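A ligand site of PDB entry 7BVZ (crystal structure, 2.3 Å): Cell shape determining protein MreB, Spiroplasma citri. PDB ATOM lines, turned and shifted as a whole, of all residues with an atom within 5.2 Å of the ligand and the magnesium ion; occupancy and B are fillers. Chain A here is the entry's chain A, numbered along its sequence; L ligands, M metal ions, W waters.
O10 of the ligand sits at hydrogen-bond distance from NZ of Lys 210 (2.4 Å).
The backbone NH (N) of Gly 159 lies within hydrogen-bond range of an oxygen (O1) of the ligand.
The backbone NH (N) of Asn 17 is in hydrogen-bond range of an oxygen (O3) of the ligand (2.9 Å).
ND2 of Asn 17 lies within hydrogen-bond range of O5 of the ligand (3.1 Å).
The backbone NH (N) of Ala 16 is in hydrogen-bond range of an oxygen (O3) of the ligand (2.9 Å).
The backbone NH (N) of Gly 287 lies within hydrogen-bond range of an oxygen (O4) of the ligand (3.1 Å).
O3 of the ligand lies within hydrogen-bond range of N of Thr 15, at 3.2 Å.
O10 of the ligand is in hydrogen-bond range of OE2 of Glu 207 (3.3 Å).
The side-chain amino group (NZ) of Lys 210 is in hydrogen-bond range of the backbone carbonyl oxygen (O) of Gly 182 (3.3 Å).
O of Gly 159 is in hydrogen-bond range of N of Asn 183, at 2.6 Å.
O of Gly 159 is in hydrogen-bond range of N of Gly 182 (3.1 Å).
The backbone NH (N) of Gly 287 is in hydrogen-bond range of the backbone carbonyl oxygen (O) of Ile 157 (3.1 Å).
OD1 of Asp 12 lies close to N of Gly 14 (3.4 Å).
The side-chain carboxylate (OE2) of Glu 207 lies within salt-bridge range of the side-chain amino group (NZ) of Lys 211, 3.4 Å away.
The backbone carbonyl oxygen (O) of Gly 158 sits at hydrogen-bond distance from the backbone NH (N) of Gly 182, at 3.1 Å.
N of Gly 288 sits at hydrogen-bond distance from O of Ile 157 (2.9 Å).
Residues that only touch the ligand: Gly 14 (3.3 Å), Ile 157 (3.9 Å), Gly 158 (3.5 Å), Lys 211 (3.7 Å), Gly 286 (3.7 Å), Gly 288 (3.8 Å), Leu 290 (3.4 Å), Ile 291 (3.5 Å) and Leu 313 (3.7 Å).
Within 4 Å of the ligand: Gly 14, Thr 15, Ala 16, Asn 17, Ile 157, Gly 158, Gly 159, Glu 207, Lys 210, Lys 211, Gly 286, Gly 287, Gly 288, Leu 290, Ile 291 and Leu 313.
The nearest printed residue that does not touch the ligand is Asn 183 (4.1 Å).
Merely in contact with the magnesium ion: Asp 156.
The magnesium ion is bound by O2 of the ligand (2.0 Å), water W1 (2.0 Å), water W5 (2.1 Å), water W7 (2.1 Å), water W9 (2.2 Å) and water W6 (2.3 Å).
The magnesium ion has six donor atoms within binding distance.
Water W9 bridges the side-chain carboxylate (OD1) of Asp 12 and the side-chain carboxylate (OE1) of Glu 134.
Water W5 lies within hydrogen-bond range of the side-chain carboxylate of Asp 156 (2.8 Å) and the side-chain carboxylate of Glu 134 (3.1 Å).
Water W3 lies within hydrogen-bond range of an oxygen (O5) of the ligand and the backbone carbonyl oxygen (O) of Leu 313.
Water W2 lies within hydrogen-bond range of the backbone carbonyl oxygen (O) of Lys 210 and a nitrogen (N4) of the ligand.
Water W13 bridges an oxygen (O4) of the ligand (2.9 Å) and the backbone carbonyl oxygen of Leu 313 (2.9 Å).
Water W4 bridges NZ of Lys 210 (2.8 Å) and N5 of the ligand (3.4 Å).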
ATOM      1  N   ASP A  12     -28.496  -1.697   8.826  1.00  0.00           N
ATOM      2  CA  ASP A  12     -28.221  -1.286   7.455  1.00  0.00           C
ATOM      3  C   ASP A  12     -26.730  -1.493   7.237  1.00  0.00           C
ATOM      4  O   ASP A  12     -25.913  -0.640   7.594  1.00  0.00           O
ATOM      5  CB  ASP A  12     -28.638   0.175   7.218  1.00  0.00           C
ATOM      6  CG  ASP A  12     -28.467   0.618   5.771  1.00  0.00           C
ATOM      7  OD1 ASP A  12     -27.783  -0.079   4.989  1.00  0.00           O
ATOM      8  OD2 ASP A  12     -29.008   1.687   5.408  1.00  0.00           O
ATOM      9  N   GLY A  14     -24.571  -1.182   4.869  1.00  0.00           N
ATOM     10  CA  GLY A  14     -24.297  -0.571   3.597  1.00  0.00           C
ATOM     11  C   GLY A  14     -22.825  -0.623   3.206  1.00  0.00           C
ATOM     12  O   GLY A  14     -21.942  -0.864   4.022  1.00  0.00           O
ATOM     13  N   THR A  15     -22.579  -0.394   1.915  1.00  0.00           N
ATOM     14  CA  THR A  15     -21.214  -0.372   1.417  1.00  0.00           C
ATOM     15  C   THR A  15     -20.434   0.825   1.961  1.00  0.00           C
ATOM     16  O   THR A  15     -19.230   0.730   2.206  1.00  0.00           O
ATOM     17  CB  THR A  15     -21.213  -0.357  -0.113  1.00  0.00           C
ATOM     18  OG1 THR A  15     -22.001  -1.451  -0.599  1.00  0.00           O
ATOM     19  CG2 THR A  15     -19.803  -0.468  -0.649  1.00  0.00           C
ATOM     20  N   ALA A  16     -21.110   1.956   2.153  1.00  0.00           N
ATOM     21  CA  ALA A  16     -20.455   3.183   2.617  1.00  0.00           C
ATOM     22  C   ALA A  16     -20.744   3.487   4.080  1.00  0.00           C
ATOM     23  O   ALA A  16     -19.833   3.910   4.808  1.00  0.00           O
ATOM     24  CB  ALA A  16     -20.884   4.369   1.752  1.00  0.00           C
ATOM     25  N   ASN A  17     -21.979   3.299   4.546  1.00  0.00           N
ATOM     26  CA  ASN A  17     -22.359   3.609   5.912  1.00  0.00           C
ATOM     27  C   ASN A  17     -23.086   2.426   6.540  1.00  0.00           C
ATOM     28  O   ASN A  17     -23.904   1.769   5.889  1.00  0.00           O
ATOM     29  CB  ASN A  17     -23.244   4.859   5.985  1.00  0.00           C
ATOM     30  CG  ASN A  17     -22.529   6.103   5.497  1.00  0.00           C
ATOM     31  OD1 ASN A  17     -21.716   6.674   6.219  1.00  0.00           O
ATOM     32  ND2 ASN A  17     -22.844   6.537   4.289  1.00  0.00           N
ATOM     33  N   GLU A 134     -34.196  -4.429   0.865  1.00  0.00           N
ATOM     34  CA  GLU A 134     -33.862  -3.040   1.142  1.00  0.00           C
ATOM     35  C   GLU A 134     -34.809  -2.076   0.430  1.00  0.00           C
ATOM     36  O   GLU A 134     -35.089  -0.994   0.948  1.00  0.00           O
ATOM     37  CB  GLU A 134     -32.424  -2.733   0.742  1.00  0.00           C
ATOM     38  CG  GLU A 134     -31.367  -3.314   1.663  1.00  0.00           C
ATOM     39  CD  GLU A 134     -29.999  -2.702   1.428  1.00  0.00           C
ATOM     40  OE1 GLU A 134     -29.215  -2.582   2.387  1.00  0.00           O
ATOM     41  OE2 GLU A 134     -29.712  -2.330   0.272  1.00  0.00           O
ATOM     42  N   ASP A 156     -32.422   3.855  -5.263  1.00  0.00           N
ATOM     43  CA  ASP A 156     -31.532   3.866  -4.109  1.00  0.00           C
ATOM     44  C   ASP A 156     -30.093   3.935  -4.613  1.00  0.00           C
ATOM     45  O   ASP A 156     -29.559   2.945  -5.119  1.00  0.00           O
ATOM     46  CB  ASP A 156     -31.752   2.620  -3.246  1.00  0.00           C
ATOM     47  CG  ASP A 156     -31.146   2.763  -1.860  1.00  0.00           C
ATOM     48  OD1 ASP A 156     -30.058   3.350  -1.730  1.00  0.00           O
ATOM     49  OD2 ASP A 156     -31.783   2.275  -0.888  1.00  0.00           O
ATOM     50  N   ILE A 157     -29.477   5.107  -4.483  1.00  0.00           N
ATOM     51  CA  ILE A 157     -28.114   5.340  -4.925  1.00  0.00           C
ATOM     52  C   ILE A 157     -27.232   5.319  -3.681  1.00  0.00           C
ATOM     53  O   ILE A 157     -27.195   6.283  -2.915  1.00  0.00           O
ATOM     54  CB  ILE A 157     -27.980   6.654  -5.689  1.00  0.00           C
ATOM     55  CG1 ILE A 157     -29.013   6.725  -6.818  1.00  0.00           C
ATOM     56  CG2 ILE A 157     -26.576   6.813  -6.252  1.00  0.00           C
ATOM     57  CD1 ILE A 157     -28.981   8.011  -7.603  1.00  0.00           C
ATOM     58  N   GLY A 158     -26.519   4.220  -3.480  1.00  0.00           N
ATOM     59  CA  GLY A 158     -25.684   4.012  -2.317  1.00  0.00           C
ATOM     60  C   GLY A 158     -24.216   4.228  -2.607  1.00  0.00           C
ATOM     61  O   GLY A 158     -23.837   5.065  -3.437  1.00  0.00           O
ATOM     62  N   GLY A 159     -23.377   3.457  -1.916  1.00  0.00           N
ATOM     63  CA  GLY A 159     -21.939   3.584  -2.074  1.00  0.00           C
ATOM     64  C   GLY A 159     -21.404   2.849  -3.293  1.00  0.00           C
ATOM     65  O   GLY A 159     -20.525   3.364  -3.996  1.00  0.00           O
ATOM     66  N   GLY A 160     -21.924   1.654  -3.547  1.00  0.00           N
ATOM     67  CA  GLY A 160     -21.422   0.866  -4.657  1.00  0.00           C
ATOM     68  C   GLY A 160     -22.499   0.263  -5.537  1.00  0.00           C
ATOM     69  O   GLY A 160     -22.197  -0.487  -6.469  1.00  0.00           O
ATOM     70  N   GLY A 182     -21.796   5.732  -5.616  1.00  0.00           N
ATOM     71  CA  GLY A 182     -20.942   6.773  -5.063  1.00  0.00           C
ATOM     72  C   GLY A 182     -19.462   6.519  -5.269  1.00  0.00           C
ATOM     73  O   GLY A 182     -18.708   7.421  -5.643  1.00  0.00           O
ATOM     74  N   ASN A 183     -19.029   5.281  -5.030  1.00  0.00           N
ATOM     75  CA  ASN A 183     -17.617   4.957  -5.222  1.00  0.00           C
ATOM     76  C   ASN A 183     -17.201   5.104  -6.678  1.00  0.00           C
ATOM     77  O   ASN A 183     -16.060   5.503  -6.969  1.00  0.00           O
ATOM     78  CB  ASN A 183     -17.329   3.533  -4.723  1.00  0.00           C
ATOM     79  CG  ASN A 183     -17.633   3.367  -3.245  1.00  0.00           C
ATOM     80  OD1 ASN A 183     -17.796   4.340  -2.518  1.00  0.00           O
ATOM     81  ND2 ASN A 183     -17.702   2.113  -2.800  1.00  0.00           N
ATOM     82  N   ASP A 186     -16.680   8.843  -7.220  1.00  0.00           N
ATOM     83  CA  ASP A 186     -15.417   9.330  -6.661  1.00  0.00           C
ATOM     84  C   ASP A 186     -14.244   8.969  -7.557  1.00  0.00           C
ATOM     85  O   ASP A 186     -13.330   9.777  -7.758  1.00  0.00           O
ATOM     86  CB  ASP A 186     -15.203   8.750  -5.259  1.00  0.00           C
ATOM     87  CG  ASP A 186     -16.368   9.047  -4.323  1.00  0.00           C
ATOM     88  OD1 ASP A 186     -17.259   9.818  -4.721  1.00  0.00           O
ATOM     89  OD2 ASP A 186     -16.372   8.499  -3.203  1.00  0.00           O
ATOM     90  N   GLU A 207     -14.216  12.437  -2.890  1.00  0.00           N
ATOM     91  CA  GLU A 207     -15.556  12.328  -2.331  1.00  0.00           C
ATOM     92  C   GLU A 207     -16.058  13.677  -1.813  1.00  0.00           C
ATOM     93  O   GLU A 207     -17.236  14.008  -1.978  1.00  0.00           O
ATOM     94  CB  GLU A 207     -15.574  11.285  -1.216  1.00  0.00           C
ATOM     95  CG  GLU A 207     -16.960  11.028  -0.640  1.00  0.00           C
ATOM     96  CD  GLU A 207     -16.955   9.994   0.472  1.00  0.00           C
ATOM     97  OE1 GLU A 207     -15.864   9.581   0.911  1.00  0.00           O
ATOM     98  OE2 GLU A 207     -18.048   9.600   0.914  1.00  0.00           O
ATOM     99  N   LYS A 210     -17.413  15.888  -4.647  1.00  0.00           N
ATOM    100  CA  LYS A 210     -18.764  15.508  -5.024  1.00  0.00           C
ATOM    101  C   LYS A 210     -19.794  16.070  -4.039  1.00  0.00           C
ATOM    102  O   LYS A 210     -20.872  16.526  -4.455  1.00  0.00           O
ATOM    103  CB  LYS A 210     -18.874  13.988  -5.112  1.00  0.00           C
ATOM    104  CG  LYS A 210     -20.265  13.458  -5.408  1.00  0.00           C
ATOM    105  CD  LYS A 210     -20.313  11.949  -5.326  1.00  0.00           C
ATOM    106  CE  LYS A 210     -19.927  11.441  -3.950  1.00  0.00           C
ATOM    107  NZ  LYS A 210     -19.939   9.957  -3.895  1.00  0.00           N
ATOM    108  N   LYS A 211     -19.477  16.054  -2.748  1.00  0.00           N
ATOM    109  CA  LYS A 211     -20.420  16.544  -1.747  1.00  0.00           C
ATOM    110  C   LYS A 211     -20.505  18.061  -1.721  1.00  0.00           C
ATOM    111  O   LYS A 211     -21.584  18.608  -1.479  1.00  0.00           O
ATOM    112  CB  LYS A 211     -20.045  16.027  -0.354  1.00  0.00           C
ATOM    113  CG  LYS A 211     -20.116  14.516  -0.198  1.00  0.00           C
ATOM    114  CD  LYS A 211     -19.672  14.107   1.200  1.00  0.00           C
ATOM    115  CE  LYS A 211     -19.757  12.604   1.401  1.00  0.00           C
ATOM    116  NZ  LYS A 211     -19.289  12.221   2.758  1.00  0.00           N
ATOM    117  N   GLY A 286     -31.154   7.485  -0.539  1.00  0.00           N
ATOM    118  CA  GLY A 286     -29.763   7.101  -0.381  1.00  0.00           C
ATOM    119  C   GLY A 286     -28.835   8.308  -0.435  1.00  0.00           C
ATOM    120  O   GLY A 286     -29.254   9.449  -0.597  1.00  0.00           O
ATOM    121  N   GLY A 287     -27.539   8.010  -0.308  1.00  0.00           N
ATOM    122  CA  GLY A 287     -26.559   9.085  -0.323  1.00  0.00           C
ATOM    123  C   GLY A 287     -26.541   9.843  -1.631  1.00  0.00           C
ATOM    124  O   GLY A 287     -26.454  11.073  -1.641  1.00  0.00           O
ATOM    125  N   GLY A 288     -26.624   9.125  -2.747  1.00  0.00           N
ATOM    126  CA  GLY A 288     -26.685   9.741  -4.064  1.00  0.00           C
ATOM    127  C   GLY A 288     -27.883  10.627  -4.297  1.00  0.00           C
ATOM    128  O   GLY A 288     -27.858  11.429  -5.245  1.00  0.00           O
ATOM    129  N   LEU A 290     -28.603  13.052  -2.546  1.00  0.00           N
ATOM    130  CA  LEU A 290     -28.187  14.383  -2.138  1.00  0.00           C
ATOM    131  C   LEU A 290     -27.451  15.148  -3.236  1.00  0.00           C
ATOM    132  O   LEU A 290     -27.039  16.293  -3.008  1.00  0.00           O
ATOM    133  CB  LEU A 290     -27.298  14.309  -0.885  1.00  0.00           C
ATOM    134  CG  LEU A 290     -27.961  14.007   0.469  1.00  0.00           C
ATOM    135  CD1 LEU A 290     -28.368  12.538   0.586  1.00  0.00           C
ATOM    136  CD2 LEU A 290     -27.029  14.387   1.605  1.00  0.00           C
ATOM    137  N   ILE A 291     -27.254  14.530  -4.407  1.00  0.00           N
ATOM    138  CA  ILE A 291     -26.695  15.262  -5.538  1.00  0.00           C
ATOM    139  C   ILE A 291     -27.604  16.424  -5.877  1.00  0.00           C
ATOM    140  O   ILE A 291     -28.825  16.255  -6.028  1.00  0.00           O
ATOM    141  CB  ILE A 291     -26.502  14.320  -6.742  1.00  0.00           C
ATOM    142  CG1 ILE A 291     -25.534  13.187  -6.412  1.00  0.00           C
ATOM    143  CG2 ILE A 291     -25.999  15.103  -7.940  1.00  0.00           C
ATOM    144  CD1 ILE A 291     -24.096  13.638  -6.265  1.00  0.00           C
ATOM    145  N   LEU A 313     -30.217   9.261   3.593  1.00  0.00           N
ATOM    146  CA  LEU A 313     -29.233   8.318   4.107  1.00  0.00           C
ATOM    147  C   LEU A 313     -29.871   7.283   5.019  1.00  0.00           C
ATOM    148  O   LEU A 313     -29.349   6.163   5.131  1.00  0.00           O
ATOM    149  CB  LEU A 313     -28.130   9.077   4.857  1.00  0.00           C
ATOM    150  CG  LEU A 313     -27.238  10.009   4.043  1.00  0.00           C
ATOM    151  CD1 LEU A 313     -26.545  11.003   4.955  1.00  0.00           C
ATOM    152  CD2 LEU A 313     -26.220   9.200   3.256  1.00  0.00           C
ATOM    153  N   VAL A 316     -33.397   3.369   4.644  1.00  0.00           N
ATOM    154  CA  VAL A 316     -33.407   1.928   4.917  1.00  0.00           C
ATOM    155  C   VAL A 316     -33.589   1.668   6.409  1.00  0.00           C
ATOM    156  O   VAL A 316     -34.396   0.826   6.814  1.00  0.00           O
ATOM    157  CB  VAL A 316     -32.128   1.271   4.373  1.00  0.00           C
ATOM    158  CG1 VAL A 316     -32.078  -0.192   4.776  1.00  0.00           C
ATOM    159  CG2 VAL A 316     -32.074   1.406   2.856  1.00  0.00           C
HETATM  160  P1  LIG L   1     -24.755   2.668   1.362  1.00  0.00           P
HETATM  161  O1  LIG L   1     -24.264   1.922   0.143  1.00  0.00           O
HETATM  162  O2  LIG L   1     -26.229   2.523   1.618  1.00  0.00           O
HETATM  163  O3  LIG L   1     -23.884   2.494   2.582  1.00  0.00           O
HETATM  164  P2  LIG L   1     -25.548   5.375   1.508  1.00  0.00           P
HETATM  165  O4  LIG L   1     -26.883   5.179   0.830  1.00  0.00           O
HETATM  166  O5  LIG L   1     -25.451   5.428   3.014  1.00  0.00           O
HETATM  167  O6  LIG L   1     -24.552   4.218   0.979  1.00  0.00           O
HETATM  168  O7  LIG L   1     -24.839   6.681   0.902  1.00  0.00           O
HETATM  169  C1  LIG L   1     -23.411   6.793   0.990  1.00  0.00           C
HETATM  170  C2  LIG L   1     -22.815   7.368  -0.291  1.00  0.00           C
HETATM  171  O8  LIG L   1     -23.500   8.541  -0.701  1.00  0.00           O
HETATM  172  C3  LIG L   1     -21.351   7.732  -0.084  1.00  0.00           C
HETATM  173  O9  LIG L   1     -20.523   6.862  -0.849  1.00  0.00           O
HETATM  174  C4  LIG L   1     -21.218   9.165  -0.557  1.00  0.00           C
HETATM  175  O10 LIG L   1     -20.224   9.251  -1.585  1.00  0.00           O
HETATM  176  C5  LIG L   1     -22.578   9.545  -1.104  1.00  0.00           C
HETATM  177  N1  LIG L   1     -22.990  10.862  -0.537  1.00  0.00           N
HETATM  178  C6  LIG L   1     -23.249  11.106   0.763  1.00  0.00           C
HETATM  179  N2  LIG L   1     -23.590  12.404   0.958  1.00  0.00           N
HETATM  180  C7  LIG L   1     -23.547  13.015  -0.235  1.00  0.00           C
HETATM  181  C8  LIG L   1     -23.798  14.384  -0.749  1.00  0.00           C
HETATM  182  N3  LIG L   1     -24.169  15.390   0.086  1.00  0.00           N
HETATM  183  N4  LIG L   1     -23.641  14.602  -2.071  1.00  0.00           N
HETATM  184  C9  LIG L   1     -23.267  13.610  -2.907  1.00  0.00           C
HETATM  185  N5  LIG L   1     -23.030  12.355  -2.522  1.00  0.00           N
HETATM  186  C10 LIG L   1     -23.144  11.992  -1.223  1.00  0.00           C
HETATM  187 MG    MG M   1     -27.932   1.603   0.982  1.00  0.00          MG
HETATM  188  O   HOH W   1     -28.488   3.417   0.229  1.00  0.00           O
HETATM  189  O   HOH W   2     -23.487  16.713  -3.919  1.00  0.00           O
HETATM  190  O   HOH W   3     -26.457   5.885   5.289  1.00  0.00           O
HETATM  191  O   HOH W   4     -22.663   9.657  -4.495  1.00  0.00           O
HETATM  192  O   HOH W   5     -29.626   0.755   0.160  1.00  0.00           O
HETATM  193  O   HOH W   6     -28.910   2.216   2.935  1.00  0.00           O
HETATM  194  O   HOH W   7     -26.771   0.525  -0.359  1.00  0.00           O
HETATM  195  O   HOH W   8     -22.140   9.256   3.036  1.00  0.00           O
HETATM  196  O   HOH W   9     -27.479  -0.196   2.203  1.00  0.00           O
HETATM  197  O   HOH W  10     -24.913  17.956  -2.043  1.00  0.00           O
HETATM  198  O   HOH W  11     -23.395  13.457   3.435  1.00  0.00           O
HETATM  199  O   HOH W  12     -24.101   7.619  -3.502  1.00  0.00           O
HETATM  200  O   HOH W  13     -29.226   5.093   2.467  1.00  0.00           O
